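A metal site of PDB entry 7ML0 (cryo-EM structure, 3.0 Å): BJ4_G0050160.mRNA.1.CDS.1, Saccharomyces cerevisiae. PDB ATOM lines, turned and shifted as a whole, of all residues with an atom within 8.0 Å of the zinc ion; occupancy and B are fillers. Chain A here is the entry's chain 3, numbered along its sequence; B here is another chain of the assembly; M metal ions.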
ATOM      1  N   MET A  12      14.720  20.468 -19.372  1.00  0.00           N
ATOM      2  CA  MET A  12      14.001  19.899 -20.499  1.00  0.00           C
ATOM      3  C   MET A  12      15.003  19.356 -21.505  1.00  0.00           C
ATOM      4  O   MET A  12      16.119  19.879 -21.641  1.00  0.00           O
ATOM      5  CB  MET A  12      13.090  20.938 -21.173  1.00  0.00           C
ATOM      6  CG  MET A  12      13.815  22.093 -21.845  1.00  0.00           C
ATOM      7  SD  MET A  12      12.687  23.292 -22.570  1.00  0.00           S
ATOM      8  CE  MET A  12      11.905  23.966 -21.110  1.00  0.00           C
ATOM      9  N   CYS A  13      14.606  18.293 -22.202  1.00  0.00           N
ATOM     10  CA  CYS A  13      15.498  17.648 -23.153  1.00  0.00           C
ATOM     11  C   CYS A  13      15.838  18.611 -24.283  1.00  0.00           C
ATOM     12  O   CYS A  13      14.921  19.143 -24.924  1.00  0.00           O
ATOM     13  CB  CYS A  13      14.854  16.385 -23.713  1.00  0.00           C
ATOM     14  SG  CYS A  13      15.836  15.550 -24.964  1.00  0.00           S
ATOM     15  N   PRO A  14      17.117  18.857 -24.554  1.00  0.00           N
ATOM     16  CA  PRO A  14      17.462  19.704 -25.711  1.00  0.00           C
ATOM     17  C   PRO A  14      16.902  19.197 -27.036  1.00  0.00           C
ATOM     18  O   PRO A  14      16.964  19.921 -28.036  1.00  0.00           O
ATOM     19  CB  PRO A  14      18.995  19.705 -25.687  1.00  0.00           C
ATOM     20  CG  PRO A  14      19.328  19.544 -24.243  1.00  0.00           C
ATOM     21  CD  PRO A  14      18.273  18.623 -23.681  1.00  0.00           C
ATOM     22  N   ILE A  15      16.374  17.982 -27.078  1.00  0.00           N
ATOM     23  CA  ILE A  15      15.835  17.430 -28.317  1.00  0.00           C
ATOM     24  C   ILE A  15      14.342  17.734 -28.410  1.00  0.00           C
ATOM     25  O   ILE A  15      13.889  18.430 -29.315  1.00  0.00           O
ATOM     26  CB  ILE A  15      16.100  15.922 -28.423  1.00  0.00           C
ATOM     27  CG1 ILE A  15      17.519  15.591 -27.983  1.00  0.00           C
ATOM     28  CG2 ILE A  15      15.852  15.438 -29.843  1.00  0.00           C
ATOM     29  CD1 ILE A  15      18.578  16.413 -28.670  1.00  0.00           C
ATOM     30  N   CYS A  16      13.567  17.194 -27.465  1.00  0.00           N
ATOM     31  CA  CYS A  16      12.125  17.354 -27.489  1.00  0.00           C
ATOM     32  C   CYS A  16      11.608  18.391 -26.504  1.00  0.00           C
ATOM     33  O   CYS A  16      10.405  18.693 -26.518  1.00  0.00           O
ATOM     34  CB  CYS A  16      11.437  16.019 -27.222  1.00  0.00           C
ATOM     35  SG  CYS A  16      12.108  15.112 -25.829  1.00  0.00           S
ATOM     36  N   LYS A  17      12.475  18.955 -25.657  1.00  0.00           N
ATOM     37  CA  LYS A  17      12.111  20.020 -24.717  1.00  0.00           C
ATOM     38  C   LYS A  17      10.938  19.606 -23.837  1.00  0.00           C
ATOM     39  O   LYS A  17      10.037  20.402 -23.548  1.00  0.00           O
ATOM     40  CB  LYS A  17      11.809  21.318 -25.459  1.00  0.00           C
ATOM     41  CG  LYS A  17      13.016  21.898 -26.188  1.00  0.00           C
ATOM     42  CD  LYS A  17      12.821  21.841 -27.692  1.00  0.00           C
ATOM     43  CE  LYS A  17      14.088  22.259 -28.442  1.00  0.00           C
ATOM     44  NZ  LYS A  17      13.882  22.220 -29.921  1.00  0.00           N
ATOM     45  N   THR A  18      10.944  18.342 -23.398  1.00  0.00           N
ATOM     46  CA  THR A  18       9.965  17.882 -22.411  1.00  0.00           C
ATOM     47  C   THR A  18      10.449  18.340 -21.045  1.00  0.00           C
ATOM     48  O   THR A  18      11.418  17.817 -20.474  1.00  0.00           O
ATOM     49  CB  THR A  18       9.779  16.370 -22.490  1.00  0.00           C
ATOM     50  OG1 THR A  18       9.052  15.925 -21.341  1.00  0.00           O
ATOM     51  CG2 THR A  18      11.108  15.647 -22.578  1.00  0.00           C
ATOM     52  N   VAL A  26      11.524  12.588 -16.079  1.00  0.00           N
ATOM     53  CA  VAL A  26      12.597  12.671 -17.053  1.00  0.00           C
ATOM     54  C   VAL A  26      13.914  12.342 -16.376  1.00  0.00           C
ATOM     55  O   VAL A  26      14.198  12.797 -15.255  1.00  0.00           O
ATOM     56  CB  VAL A  26      12.630  14.061 -17.721  1.00  0.00           C
ATOM     57  CG1 VAL A  26      12.951  15.155 -16.703  1.00  0.00           C
ATOM     58  CG2 VAL A  26      13.634  14.073 -18.859  1.00  0.00           C
ATOM     59  N   PHE A  28      17.961  12.363 -17.263  1.00  0.00           N
ATOM     60  CA  PHE A  28      18.899  12.830 -18.257  1.00  0.00           C
ATOM     61  C   PHE A  28      20.145  11.961 -18.242  1.00  0.00           C
ATOM     62  O   PHE A  28      20.627  11.541 -17.195  1.00  0.00           O
ATOM     63  CB  PHE A  28      19.263  14.286 -18.015  1.00  0.00           C
ATOM     64  CG  PHE A  28      18.261  15.247 -18.566  1.00  0.00           C
ATOM     65  CD1 PHE A  28      18.451  15.821 -19.815  1.00  0.00           C
ATOM     66  CD2 PHE A  28      17.123  15.563 -17.852  1.00  0.00           C
ATOM     67  CE1 PHE A  28      17.526  16.701 -20.330  1.00  0.00           C
ATOM     68  CE2 PHE A  28      16.192  16.446 -18.359  1.00  0.00           C
ATOM     69  CZ  PHE A  28      16.387  17.014 -19.602  1.00  0.00           C
ATOM     70  N   ARG A  37      23.164  16.777 -23.013  1.00  0.00           N
ATOM     71  CA  ARG A  37      21.935  16.715 -22.251  1.00  0.00           C
ATOM     72  C   ARG A  37      20.799  16.204 -23.118  1.00  0.00           C
ATOM     73  O   ARG A  37      20.608  16.675 -24.249  1.00  0.00           O
ATOM     74  CB  ARG A  37      21.597  18.096 -21.679  1.00  0.00           C
ATOM     75  CG  ARG A  37      22.683  18.657 -20.789  1.00  0.00           C
ATOM     76  CD  ARG A  37      22.102  19.546 -19.701  1.00  0.00           C
ATOM     77  NE  ARG A  37      21.373  18.788 -18.686  1.00  0.00           N
ATOM     78  CZ  ARG A  37      20.060  18.593 -18.694  1.00  0.00           C
ATOM     79  NH1 ARG A  37      19.318  19.107 -19.668  1.00  0.00           N
ATOM     80  NH2 ARG A  37      19.485  17.901 -17.725  1.00  0.00           N
ATOM     81  N   ILE A  38      20.064  15.216 -22.610  1.00  0.00           N
ATOM     82  CA  ILE A  38      19.009  14.583 -23.384  1.00  0.00           C
ATOM     83  C   ILE A  38      18.180  13.712 -22.447  1.00  0.00           C
ATOM     84  O   ILE A  38      18.691  13.199 -21.444  1.00  0.00           O
ATOM     85  CB  ILE A  38      19.588  13.762 -24.553  1.00  0.00           C
ATOM     86  CG1 ILE A  38      18.488  13.274 -25.495  1.00  0.00           C
ATOM     87  CG2 ILE A  38      20.380  12.574 -24.035  1.00  0.00           C
ATOM     88  CD1 ILE A  38      19.041  12.616 -26.737  1.00  0.00           C
ATOM     89  N   CYS A  39      16.897  13.572 -22.753  1.00  0.00           N
ATOM     90  CA  CYS A  39      16.051  12.634 -22.022  1.00  0.00           C
ATOM     91  C   CYS A  39      16.261  11.216 -22.529  1.00  0.00           C
ATOM     92  O   CYS A  39      16.653  10.971 -23.677  1.00  0.00           O
ATOM     93  CB  CYS A  39      14.581  13.032 -22.163  1.00  0.00           C
ATOM     94  SG  CYS A  39      13.874  12.628 -23.764  1.00  0.00           S
ATOM     95  N   GLU A  40      15.975  10.251 -21.643  1.00  0.00           N
ATOM     96  CA  GLU A  40      16.123   8.844 -22.005  1.00  0.00           C
ATOM     97  C   GLU A  40      15.184   8.467 -23.135  1.00  0.00           C
ATOM     98  O   GLU A  40      15.490   7.582 -23.943  1.00  0.00           O
ATOM     99  CB  GLU A  40      15.874   7.960 -20.789  1.00  0.00           C
ATOM    100  CG  GLU A  40      16.994   7.980 -19.786  1.00  0.00           C
ATOM    101  CD  GLU A  40      16.664   7.195 -18.538  1.00  0.00           C
ATOM    102  OE1 GLU A  40      15.462   7.144 -18.176  1.00  0.00           O
ATOM    103  OE2 GLU A  40      17.579   6.620 -17.934  1.00  0.00           O
ATOM    104  N   SER A  41      14.018   9.124 -23.201  1.00  0.00           N
ATOM    105  CA  SER A  41      13.049   8.822 -24.253  1.00  0.00           C
ATOM    106  C   SER A  41      13.705   8.872 -25.629  1.00  0.00           C
ATOM    107  O   SER A  41      13.553   7.956 -26.443  1.00  0.00           O
ATOM    108  CB  SER A  41      11.874   9.801 -24.184  1.00  0.00           C
ATOM    109  OG  SER A  41      11.892  10.684 -25.293  1.00  0.00           O
ATOM    110  N   CYS A  42      14.448   9.954 -25.897  1.00  0.00           N
ATOM    111  CA  CYS A  42      15.239  10.009 -27.114  1.00  0.00           C
ATOM    112  C   CYS A  42      16.335   8.950 -27.104  1.00  0.00           C
ATOM    113  O   CYS A  42      16.558   8.257 -28.101  1.00  0.00           O
ATOM    114  CB  CYS A  42      15.827  11.408 -27.284  1.00  0.00           C
ATOM    115  SG  CYS A  42      14.612  12.733 -27.449  1.00  0.00           S
ATOM    116  N   VAL A  43      17.018   8.794 -25.968  1.00  0.00           N
ATOM    117  CA  VAL A  43      18.177   7.910 -25.841  1.00  0.00           C
ATOM    118  C   VAL A  43      17.856   6.538 -26.383  1.00  0.00           C
ATOM    119  O   VAL A  43      18.559   6.019 -27.263  1.00  0.00           O
ATOM    120  CB  VAL A  43      18.634   7.801 -24.380  1.00  0.00           C
ATOM    121  CG1 VAL A  43      19.579   6.617 -24.220  1.00  0.00           C
ATOM    122  CG2 VAL A  43      19.284   9.089 -23.916  1.00  0.00           C
ATOM    123  N   ILE A  46      16.780   6.774 -30.063  1.00  0.00           N
ATOM    124  CA  ILE A  46      17.940   7.060 -30.901  1.00  0.00           C
ATOM    125  C   ILE A  46      18.793   5.821 -31.109  1.00  0.00           C
ATOM    126  O   ILE A  46      19.211   5.524 -32.230  1.00  0.00           O
ATOM    127  CB  ILE A  46      18.747   8.221 -30.286  1.00  0.00           C
ATOM    128  CG1 ILE A  46      18.120   9.554 -30.693  1.00  0.00           C
ATOM    129  CG2 ILE A  46      20.208   8.156 -30.740  1.00  0.00           C
ATOM    130  CD1 ILE A  46      18.157   9.813 -32.183  1.00  0.00           C
ATOM    131  N   PRO A  55      21.814  12.769 -31.637  1.00  0.00           N
ATOM    132  CA  PRO A  55      20.707  13.604 -32.096  1.00  0.00           C
ATOM    133  C   PRO A  55      20.870  15.076 -31.758  1.00  0.00           C
ATOM    134  O   PRO A  55      19.963  15.731 -31.236  1.00  0.00           O
ATOM    135  CB  PRO A  55      19.499  13.011 -31.362  1.00  0.00           C
ATOM    136  CG  PRO A  55      20.087  12.481 -30.104  1.00  0.00           C
ATOM    137  CD  PRO A  55      21.409  11.898 -30.513  1.00  0.00           C
ATOM    138  N   LYS B 110       3.749  12.600 -28.194  1.00  0.00           N
ATOM    139  CA  LYS B 110       4.635  11.630 -27.580  1.00  0.00           C
ATOM    140  C   LYS B 110       4.458  10.248 -28.210  1.00  0.00           C
ATOM    141  O   LYS B 110       5.438   9.532 -28.435  1.00  0.00           O
ATOM    142  CB  LYS B 110       4.384  11.568 -26.076  1.00  0.00           C
ATOM    143  CG  LYS B 110       5.650  11.348 -25.273  1.00  0.00           C
ATOM    144  CD  LYS B 110       6.710  12.345 -25.706  1.00  0.00           C
ATOM    145  CE  LYS B 110       8.107  11.856 -25.373  1.00  0.00           C
ATOM    146  NZ  LYS B 110       9.142  12.734 -25.971  1.00  0.00           N
ATOM    147  N   LEU B 113       6.012  10.362 -31.935  1.00  0.00           N
ATOM    148  CA  LEU B 113       7.455  10.246 -32.161  1.00  0.00           C
ATOM    149  C   LEU B 113       7.795   8.922 -32.845  1.00  0.00           C
ATOM    150  O   LEU B 113       8.812   8.817 -33.537  1.00  0.00           O
ATOM    151  CB  LEU B 113       8.202  10.380 -30.837  1.00  0.00           C
ATOM    152  CG  LEU B 113       9.737  10.440 -30.939  1.00  0.00           C
ATOM    153  CD1 LEU B 113      10.197  11.843 -31.280  1.00  0.00           C
ATOM    154  CD2 LEU B 113      10.401   9.939 -29.676  1.00  0.00           C
HETATM  155 ZN    ZN M   1      14.160  14.054 -25.574  1.00  0.00          ZN
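CB of Ile 15 touches the zinc ion, at 3.9 Å. The nearest printed residue that does not touch the zinc ion is Ser 41 (4.1 Å).
SG of Cys 39 lies close to OG of Ser 41. The side-chain sulfur (SG) of Cys 13 sits close to the backbone NH (N) of Ile 15 (3.3 Å).
SG of Cys 39 binds the zinc ion, 2.3 Å away. SG of Cys 16 binds the zinc ion, 2.3 Å away. The side-chain sulfur (SG) of Cys 13 binds the zinc ion (2.3 Å). The zinc ion is bound by SG of Cys 42, 2.3 Å away.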
